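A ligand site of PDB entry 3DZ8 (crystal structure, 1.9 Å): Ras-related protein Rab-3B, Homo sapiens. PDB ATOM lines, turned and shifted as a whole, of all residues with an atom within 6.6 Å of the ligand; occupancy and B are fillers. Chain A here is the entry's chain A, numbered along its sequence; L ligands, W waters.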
ATOM      1  N   GLY A  30      -9.537 -18.868 -30.476  1.00  0.00           N
ATOM      2  CA  GLY A  30     -10.149 -19.135 -29.185  1.00  0.00           C
ATOM      3  C   GLY A  30     -11.532 -19.760 -29.337  1.00  0.00           C
ATOM      4  O   GLY A  30     -12.120 -19.806 -30.434  1.00  0.00           O
ATOM      5  N   ASN A  31     -12.086 -20.205 -28.224  1.00  0.00           N
ATOM      6  CA  ASN A  31     -13.406 -20.853 -28.239  1.00  0.00           C
ATOM      7  C   ASN A  31     -14.487 -19.976 -28.833  1.00  0.00           C
ATOM      8  O   ASN A  31     -14.410 -18.748 -28.772  1.00  0.00           O
ATOM      9  CB  ASN A  31     -13.818 -21.304 -26.834  1.00  0.00           C
ATOM     10  CG  ASN A  31     -13.179 -22.590 -26.436  1.00  0.00           C
ATOM     11  OD1 ASN A  31     -12.188 -22.999 -27.040  1.00  0.00           O
ATOM     12  ND2 ASN A  31     -13.721 -23.254 -25.414  1.00  0.00           N
ATOM     13  N   SER A  32     -15.484 -20.632 -29.429  1.00  0.00           N
ATOM     14  CA  SER A  32     -16.682 -19.966 -29.886  1.00  0.00           C
ATOM     15  C   SER A  32     -17.221 -19.151 -28.744  1.00  0.00           C
ATOM     16  O   SER A  32     -17.270 -19.625 -27.587  1.00  0.00           O
ATOM     17  CB  SER A  32     -17.746 -20.982 -30.311  1.00  0.00           C
ATOM     18  OG  SER A  32     -17.278 -21.857 -31.339  1.00  0.00           O
ATOM     19  N   SER A  33     -17.575 -17.931 -29.063  1.00  0.00           N
ATOM     20  CA  SER A  33     -18.350 -17.068 -28.214  1.00  0.00           C
ATOM     21  C   SER A  33     -17.522 -16.346 -27.116  1.00  0.00           C
ATOM     22  O   SER A  33     -18.100 -15.658 -26.267  1.00  0.00           O
ATOM     23  CB  SER A  33     -19.547 -17.846 -27.652  1.00  0.00           C
ATOM     24  OG  SER A  33     -20.524 -16.955 -27.190  1.00  0.00           O
ATOM     25  N   VAL A  34     -16.184 -16.438 -27.182  1.00  0.00           N
ATOM     26  CA  VAL A  34     -15.322 -15.644 -26.281  1.00  0.00           C
ATOM     27  C   VAL A  34     -15.234 -14.121 -26.636  1.00  0.00           C
ATOM     28  O   VAL A  34     -14.774 -13.319 -25.821  1.00  0.00           O
ATOM     29  CB  VAL A  34     -13.934 -16.259 -26.163  1.00  0.00           C
ATOM     30  CG1 VAL A  34     -14.062 -17.763 -25.733  1.00  0.00           C
ATOM     31  CG2 VAL A  34     -13.131 -16.096 -27.473  1.00  0.00           C
ATOM     32  N   GLY A  35     -15.650 -13.728 -27.841  1.00  0.00           N
ATOM     33  CA  GLY A  35     -15.644 -12.323 -28.256  1.00  0.00           C
ATOM     34  C   GLY A  35     -14.646 -11.935 -29.350  1.00  0.00           C
ATOM     35  O   GLY A  35     -14.316 -10.749 -29.482  1.00  0.00           O
ATOM     36  N   LYS A  36     -14.180 -12.923 -30.107  1.00  0.00           N
ATOM     37  CA  LYS A  36     -13.210 -12.706 -31.185  1.00  0.00           C
ATOM     38  C   LYS A  36     -13.725 -11.713 -32.222  1.00  0.00           C
ATOM     39  O   LYS A  36     -13.051 -10.740 -32.558  1.00  0.00           O
ATOM     40  CB  LYS A  36     -12.853 -14.023 -31.873  1.00  0.00           C
ATOM     41  CG  LYS A  36     -12.171 -15.047 -30.939  1.00  0.00           C
ATOM     42  CD  LYS A  36     -11.742 -16.315 -31.669  1.00  0.00           C
ATOM     43  CE  LYS A  36     -12.941 -17.076 -32.340  1.00  0.00           C
ATOM     44  NZ  LYS A  36     -14.070 -17.550 -31.396  1.00  0.00           N
ATOM     45  N   THR A  37     -14.928 -11.947 -32.726  1.00  0.00           N
ATOM     46  CA  THR A  37     -15.519 -11.083 -33.733  1.00  0.00           C
ATOM     47  C   THR A  37     -15.717  -9.687 -33.176  1.00  0.00           C
ATOM     48  O   THR A  37     -15.377  -8.674 -33.816  1.00  0.00           O
ATOM     49  CB  THR A  37     -16.878 -11.645 -34.184  1.00  0.00           C
ATOM     50  OG1 THR A  37     -16.714 -13.012 -34.615  1.00  0.00           O
ATOM     51  CG2 THR A  37     -17.466 -10.790 -35.285  1.00  0.00           C
ATOM     52  N   SER A  38     -16.230  -9.644 -31.951  1.00  0.00           N
ATOM     53  CA  SER A  38     -16.499  -8.368 -31.280  1.00  0.00           C
ATOM     54  C   SER A  38     -15.214  -7.552 -31.115  1.00  0.00           C
ATOM     55  O   SER A  38     -15.201  -6.339 -31.327  1.00  0.00           O
ATOM     56  CB  SER A  38     -17.163  -8.604 -29.920  1.00  0.00           C
ATOM     57  OG  SER A  38     -18.458  -9.130 -30.098  1.00  0.00           O
ATOM     58  N   PHE A  39     -14.146  -8.254 -30.775  1.00  0.00           N
ATOM     59  CA  PHE A  39     -12.833  -7.679 -30.540  1.00  0.00           C
ATOM     60  C   PHE A  39     -12.257  -7.142 -31.857  1.00  0.00           C
ATOM     61  O   PHE A  39     -11.812  -5.998 -31.921  1.00  0.00           O
ATOM     62  CB  PHE A  39     -11.958  -8.782 -29.960  1.00  0.00           C
ATOM     63  CG  PHE A  39     -10.706  -8.311 -29.309  1.00  0.00           C
ATOM     64  CD1 PHE A  39     -10.693  -8.029 -27.949  1.00  0.00           C
ATOM     65  CD2 PHE A  39      -9.541  -8.162 -30.019  1.00  0.00           C
ATOM     66  CE1 PHE A  39      -9.543  -7.597 -27.320  1.00  0.00           C
ATOM     67  CE2 PHE A  39      -8.376  -7.740 -29.375  1.00  0.00           C
ATOM     68  CZ  PHE A  39      -8.397  -7.467 -28.025  1.00  0.00           C
ATOM     69  N   LYS A  63     -13.671 -13.548 -41.247  1.00  0.00           N
ATOM     70  CA  LYS A  63     -13.837 -12.119 -40.961  1.00  0.00           C
ATOM     71  C   LYS A  63     -12.458 -11.521 -41.028  1.00  0.00           C
ATOM     72  O   LYS A  63     -11.528 -12.006 -40.328  1.00  0.00           O
ATOM     73  CB  LYS A  63     -14.436 -11.936 -39.582  1.00  0.00           C
ATOM     74  CG  LYS A  63     -15.813 -12.535 -39.474  1.00  0.00           C
ATOM     75  CD  LYS A  63     -16.172 -12.916 -38.105  1.00  0.00           C
ATOM     76  CE  LYS A  63     -17.634 -13.392 -38.043  1.00  0.00           C
ATOM     77  NZ  LYS A  63     -17.817 -14.295 -36.863  1.00  0.00           N
ATOM     78  N   ILE A  76     -10.189 -13.751 -38.583  1.00  0.00           N
ATOM     79  CA  ILE A  76     -10.880 -14.760 -37.825  1.00  0.00           C
ATOM     80  C   ILE A  76     -11.391 -15.768 -38.837  1.00  0.00           C
ATOM     81  O   ILE A  76     -11.965 -15.386 -39.837  1.00  0.00           O
ATOM     82  CB  ILE A  76     -12.100 -14.209 -37.086  1.00  0.00           C
ATOM     83  CG1 ILE A  76     -11.678 -13.290 -35.954  1.00  0.00           C
ATOM     84  CG2 ILE A  76     -12.985 -15.342 -36.479  1.00  0.00           C
ATOM     85  CD1 ILE A  76     -12.799 -12.468 -35.449  1.00  0.00           C
ATOM     86  N   ASP A  78     -13.854 -18.837 -38.076  1.00  0.00           N
ATOM     87  CA  ASP A  78     -14.649 -19.299 -36.930  1.00  0.00           C
ATOM     88  C   ASP A  78     -14.169 -20.674 -36.433  1.00  0.00           C
ATOM     89  O   ASP A  78     -13.859 -21.559 -37.224  1.00  0.00           O
ATOM     90  CB  ASP A  78     -16.127 -19.469 -37.307  1.00  0.00           C
ATOM     91  CG  ASP A  78     -16.883 -18.154 -37.439  1.00  0.00           C
ATOM     92  OD1 ASP A  78     -16.364 -17.078 -37.055  1.00  0.00           O
ATOM     93  OD2 ASP A  78     -18.027 -18.258 -37.958  1.00  0.00           O
ATOM     94  N   THR A  79     -14.169 -20.840 -35.128  1.00  0.00           N
ATOM     95  CA  THR A  79     -13.798 -22.105 -34.480  1.00  0.00           C
ATOM     96  C   THR A  79     -14.614 -23.295 -34.974  1.00  0.00           C
ATOM     97  O   THR A  79     -14.066 -24.382 -35.224  1.00  0.00           O
ATOM     98  CB  THR A  79     -13.925 -21.963 -32.954  1.00  0.00           C
ATOM     99  OG1 THR A  79     -12.998 -20.964 -32.498  1.00  0.00           O
ATOM    100  CG2 THR A  79     -13.710 -23.326 -32.228  1.00  0.00           C
ATOM    101  N   MET A 102      -7.584 -15.931 -27.402  1.00  0.00           N
ATOM    102  CA  MET A 102      -8.625 -15.314 -26.559  1.00  0.00           C
ATOM    103  C   MET A 102      -9.403 -16.341 -25.743  1.00  0.00           C
ATOM    104  O   MET A 102      -9.760 -17.429 -26.250  1.00  0.00           O
ATOM    105  CB  MET A 102      -9.603 -14.516 -27.427  1.00  0.00           C
ATOM    106  CG  MET A 102     -10.533 -13.590 -26.613  1.00  0.00           C
ATOM    107  SD  MET A 102     -11.521 -12.471 -27.597  1.00  0.00           S
ATOM    108  CE  MET A 102     -10.282 -11.798 -28.666  1.00  0.00           C
ATOM    109  N   ASP A 104     -12.571 -16.082 -22.341  1.00  0.00           N
ATOM    110  CA  ASP A 104     -13.606 -15.262 -21.758  1.00  0.00           C
ATOM    111  C   ASP A 104     -13.453 -15.414 -20.228  1.00  0.00           C
ATOM    112  O   ASP A 104     -13.541 -16.530 -19.719  1.00  0.00           O
ATOM    113  CB  ASP A 104     -14.940 -15.792 -22.300  1.00  0.00           C
ATOM    114  CG  ASP A 104     -16.176 -15.180 -21.649  1.00  0.00           C
ATOM    115  OD1 ASP A 104     -16.101 -14.404 -20.654  1.00  0.00           O
ATOM    116  OD2 ASP A 104     -17.252 -15.525 -22.142  1.00  0.00           O
ATOM    117  N   ASN A 136     -10.805 -11.840 -22.387  1.00  0.00           N
ATOM    118  CA  ASN A 136     -11.818 -10.887 -22.833  1.00  0.00           C
ATOM    119  C   ASN A 136     -13.048 -10.818 -21.901  1.00  0.00           C
ATOM    120  O   ASN A 136     -13.254 -11.696 -21.069  1.00  0.00           O
ATOM    121  CB  ASN A 136     -12.280 -11.231 -24.257  1.00  0.00           C
ATOM    122  CG  ASN A 136     -13.130 -10.159 -24.855  1.00  0.00           C
ATOM    123  OD1 ASN A 136     -12.845  -8.966 -24.660  1.00  0.00           O
ATOM    124  ND2 ASN A 136     -14.217 -10.541 -25.554  1.00  0.00           N
ATOM    125  N   LYS A 137     -13.842  -9.772 -22.078  1.00  0.00           N
ATOM    126  CA  LYS A 137     -15.091  -9.541 -21.315  1.00  0.00           C
ATOM    127  C   LYS A 137     -14.766  -9.075 -19.899  1.00  0.00           C
ATOM    128  O   LYS A 137     -15.536  -9.324 -18.956  1.00  0.00           O
ATOM    129  CB  LYS A 137     -16.033 -10.776 -21.299  1.00  0.00           C
ATOM    130  CG  LYS A 137     -16.342 -11.403 -22.691  1.00  0.00           C
ATOM    131  CD  LYS A 137     -17.662 -12.200 -22.730  1.00  0.00           C
ATOM    132  CE  LYS A 137     -17.744 -13.032 -23.986  1.00  0.00           C
ATOM    133  NZ  LYS A 137     -18.925 -13.932 -24.048  1.00  0.00           N
ATOM    134  N   CYS A 138     -13.643  -8.356 -19.749  1.00  0.00           N
ATOM    135  CA  CYS A 138     -13.221  -7.880 -18.426  1.00  0.00           C
ATOM    136  C   CYS A 138     -14.175  -6.831 -17.864  1.00  0.00           C
ATOM    137  O   CYS A 138     -14.142  -6.536 -16.676  1.00  0.00           O
ATOM    138  CB  CYS A 138     -11.766  -7.384 -18.445  1.00  0.00           C
ATOM    139  SG  CYS A 138     -11.500  -5.779 -19.177  1.00  0.00           S
ATOM    140  N   ASP A 139     -15.066  -6.284 -18.711  1.00  0.00           N
ATOM    141  CA  ASP A 139     -16.174  -5.442 -18.231  1.00  0.00           C
ATOM    142  C   ASP A 139     -17.183  -6.197 -17.328  1.00  0.00           C
ATOM    143  O   ASP A 139     -17.902  -5.554 -16.563  1.00  0.00           O
ATOM    144  CB  ASP A 139     -16.929  -4.824 -19.390  1.00  0.00           C
ATOM    145  CG  ASP A 139     -17.551  -5.872 -20.316  1.00  0.00           C
ATOM    146  OD1 ASP A 139     -16.791  -6.606 -20.981  1.00  0.00           O
ATOM    147  OD2 ASP A 139     -18.797  -5.950 -20.386  1.00  0.00           O
ATOM    148  N   MET A 140     -17.229  -7.525 -17.422  1.00  0.00           N
ATOM    149  CA  MET A 140     -18.222  -8.318 -16.672  1.00  0.00           C
ATOM    150  C   MET A 140     -17.647  -8.865 -15.352  1.00  0.00           C
ATOM    151  O   MET A 140     -17.714 -10.057 -15.112  1.00  0.00           O
ATOM    152  CB  MET A 140     -18.721  -9.489 -17.534  1.00  0.00           C
ATOM    153  CG  MET A 140     -19.362  -9.071 -18.857  1.00  0.00           C
ATOM    154  SD  MET A 140     -20.780  -7.980 -18.612  1.00  0.00           S
ATOM    155  CE  MET A 140     -21.908  -9.052 -17.711  1.00  0.00           C
ATOM    156  N   ALA A 165      -9.026  -7.622 -21.402  1.00  0.00           N
ATOM    157  CA  ALA A 165      -9.549  -6.651 -22.332  1.00  0.00           C
ATOM    158  C   ALA A 165     -11.056  -6.695 -22.332  1.00  0.00           C
ATOM    159  O   ALA A 165     -11.664  -7.593 -21.754  1.00  0.00           O
ATOM    160  CB  ALA A 165      -8.991  -6.912 -23.742  1.00  0.00           C
ATOM    161  N   SER A 166     -11.663  -5.697 -22.954  1.00  0.00           N
ATOM    162  CA  SER A 166     -13.087  -5.670 -23.166  1.00  0.00           C
ATOM    163  C   SER A 166     -13.357  -5.098 -24.548  1.00  0.00           C
ATOM    164  O   SER A 166     -13.116  -3.928 -24.799  1.00  0.00           O
ATOM    165  CB  SER A 166     -13.806  -4.831 -22.135  1.00  0.00           C
ATOM    166  OG  SER A 166     -15.194  -4.693 -22.503  1.00  0.00           O
ATOM    167  N   ALA A 167     -13.879  -5.958 -25.428  1.00  0.00           N
ATOM    168  CA  ALA A 167     -14.365  -5.532 -26.757  1.00  0.00           C
ATOM    169  C   ALA A 167     -15.532  -4.574 -26.613  1.00  0.00           C
ATOM    170  O   ALA A 167     -15.642  -3.592 -27.356  1.00  0.00           O
ATOM    171  CB  ALA A 167     -14.793  -6.745 -27.558  1.00  0.00           C
ATOM    172  N   LYS A 168     -16.395  -4.832 -25.631  1.00  0.00           N
ATOM    173  CA  LYS A 168     -17.610  -4.014 -25.432  1.00  0.00           C
ATOM    174  C   LYS A 168     -17.280  -2.616 -24.891  1.00  0.00           C
ATOM    175  O   LYS A 168     -17.902  -1.630 -25.289  1.00  0.00           O
ATOM    176  CB  LYS A 168     -18.597  -4.720 -24.494  1.00  0.00           C
ATOM    177  CG  LYS A 168     -19.702  -3.788 -23.940  1.00  0.00           C
ATOM    178  N   GLU A 169     -16.297  -2.554 -24.009  1.00  0.00           N
ATOM    179  CA  GLU A 169     -15.889  -1.319 -23.379  1.00  0.00           C
ATOM    180  C   GLU A 169     -14.649  -0.702 -23.999  1.00  0.00           C
ATOM    181  O   GLU A 169     -14.178   0.294 -23.529  1.00  0.00           O
ATOM    182  CB  GLU A 169     -15.645  -1.542 -21.889  1.00  0.00           C
ATOM    183  CG  GLU A 169     -16.906  -1.861 -21.111  1.00  0.00           C
ATOM    184  CD  GLU A 169     -17.861  -0.685 -21.069  1.00  0.00           C
ATOM    185  OE1 GLU A 169     -17.445   0.412 -20.612  1.00  0.00           O
ATOM    186  OE2 GLU A 169     -19.027  -0.840 -21.488  1.00  0.00           O
HETATM  187  P1  LIG L   1     -16.842 -15.195 -31.153  1.00  0.00           P
HETATM  188  O1  LIG L   1     -16.519 -14.454 -32.452  1.00  0.00           O
HETATM  189  O2  LIG L   1     -17.710 -16.368 -31.410  1.00  0.00           O
HETATM  190  O3  LIG L   1     -15.598 -15.606 -30.390  1.00  0.00           O
HETATM  191  O4  LIG L   1     -17.606 -14.226 -30.106  1.00  0.00           O
HETATM  192  P2  LIG L   1     -18.548 -12.985 -30.464  1.00  0.00           P
HETATM  193  O5  LIG L   1     -17.816 -11.683 -30.759  1.00  0.00           O
HETATM  194  O6  LIG L   1     -19.638 -13.414 -31.446  1.00  0.00           O
HETATM  195  O7  LIG L   1     -19.245 -12.692 -29.032  1.00  0.00           O
HETATM  196  C1  LIG L   1     -20.008 -13.717 -28.409  1.00  0.00           C
HETATM  197  C2  LIG L   1     -20.937 -13.115 -27.370  1.00  0.00           C
HETATM  198  O8  LIG L   1     -20.150 -12.461 -26.366  1.00  0.00           O
HETATM  199  C3  LIG L   1     -21.802 -12.052 -28.017  1.00  0.00           C
HETATM  200  O9  LIG L   1     -23.093 -11.987 -27.422  1.00  0.00           O
HETATM  201  C4  LIG L   1     -21.078 -10.757 -27.724  1.00  0.00           C
HETATM  202  O10 LIG L   1     -21.946  -9.643 -27.668  1.00  0.00           O
HETATM  203  C5  LIG L   1     -20.462 -11.066 -26.349  1.00  0.00           C
HETATM  204  N1  LIG L   1     -19.246 -10.299 -26.101  1.00  0.00           N
HETATM  205  C6  LIG L   1     -18.153 -10.257 -26.906  1.00  0.00           C
HETATM  206  N2  LIG L   1     -17.190  -9.460 -26.392  1.00  0.00           N
HETATM  207  C7  LIG L   1     -17.670  -8.987 -25.211  1.00  0.00           C
HETATM  208  C8  LIG L   1     -17.152  -8.119 -24.140  1.00  0.00           C
HETATM  209  O11 LIG L   1     -16.049  -7.577 -24.217  1.00  0.00           O
HETATM  210  N3  LIG L   1     -17.952  -7.880 -23.075  1.00  0.00           N
HETATM  211  C9  LIG L   1     -19.185  -8.420 -22.979  1.00  0.00           C
HETATM  212  N4  LIG L   1     -19.928  -8.151 -21.899  1.00  0.00           N
HETATM  213  N5  LIG L   1     -19.711  -9.249 -23.910  1.00  0.00           N
HETATM  214  C10 LIG L   1     -19.012  -9.547 -25.029  1.00  0.00           C
HETATM  215  O   HOH W   1     -15.563 -16.305 -34.441  1.00  0.00           O
HETATM  216  O   HOH W   2     -23.538 -12.863 -24.843  1.00  0.00           O
HETATM  217  O   HOH W   3     -19.833 -14.258 -33.954  1.00  0.00           O
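The backbone NH (N) of Thr 37 is in hydrogen-bond range of an oxygen (O1) of the ligand (3.0 Å). The side-chain hydroxyl of Thr 37 is in hydrogen-bond range of an oxygen (O1) of the ligand. O3 of the ligand lies within hydrogen-bond range of N of Lys 36, 3.0 Å away. O3 of the ligand lies within salt-bridge range of NZ of Lys 36 (2.7 Å). N3 of the ligand lies within hydrogen-bond range of OD1 of Asp 139, 2.7 Å away. An oxygen (O5) of the ligand is in hydrogen-bond range of the backbone NH (N) of Ser 38 (2.8 Å). An oxygen (O5) of the ligand sits at hydrogen-bond distance from the side-chain hydroxyl of Ser 38 (2.7 Å). O2 of the ligand sits at hydrogen-bond distance from N of Ser 33 (2.8 Å). O11 of the ligand is in hydrogen-bond range of N of Ala 167 (3.0 Å). The side-chain amino group of Lys 137 lies within hydrogen-bond range of an oxygen (O8) of the ligand, at 3.0 Å. The backbone NH of Gly 35 is in hydrogen-bond range of an oxygen (O4) of the ligand. O11 of the ligand sits at hydrogen-bond distance from N of Lys 168 (3.1 Å). N4 of the ligand sits close to SD of Met 140, 3.4 Å away. N2 of the ligand is in hydrogen-bond range of ND2 of Asn 136, at 3.3 Å. An oxygen (O3) of the ligand sits at hydrogen-bond distance from the backbone NH (N) of Val 34 (3.4 Å). The side-chain hydroxyl (OG) of Ser 166 sits at hydrogen-bond distance from an oxygen (O11) of the ligand (3.5 Å).
Water W3 bridges an oxygen (O6) of the ligand (2.7 Å) and the side-chain hydroxyl of Thr 37 (3.4 Å). Water W1 lies within hydrogen-bond range of OD1 of Asp 78, O1 of the ligand and OG1 of Thr 37.
The side-chain hydroxyl of Thr 37 lies within hydrogen-bond range of the side-chain amino group of Lys 63 (2.8 Å). OD1 of Asp 139 lies within hydrogen-bond range of OG of Ser 166, 2.9 Å away. N of Ala 167 lies within hydrogen-bond range of OD1 of Asn 136, 3.3 Å away. The backbone NH of Lys 137 lies within hydrogen-bond range of the backbone carbonyl oxygen of Ala 165 (3.1 Å). O of Val 34 is in hydrogen-bond range of ND2 of Asn 136. OD1 of Asn 136 lies close to O of Ala 165, 3.4 Å away. The side-chain hydroxyl (OG) of Ser 166 sits at hydrogen-bond distance from the backbone NH (N) of Glu 169 (2.8 Å). N of Ser 166 lies within hydrogen-bond range of SG of Cys 138 (3.8 Å).
O of Asn 31 touches O3 of the ligand, 3.7 Å away. Ser 32 touches the ligand. Hydrophobic or aromatic side chains within 4 Å of the ligand: Val 34, Met 140 and Ala 167. Within 4 Å of the ligand: Asn 31, Ser 32, Ser 33, Val 34, Gly 35, Lys 36, Thr 37, Ser 38, Asn 136, Lys 137, Asp 139, Met 140, Ser 166, Ala 167 and Lys 168.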
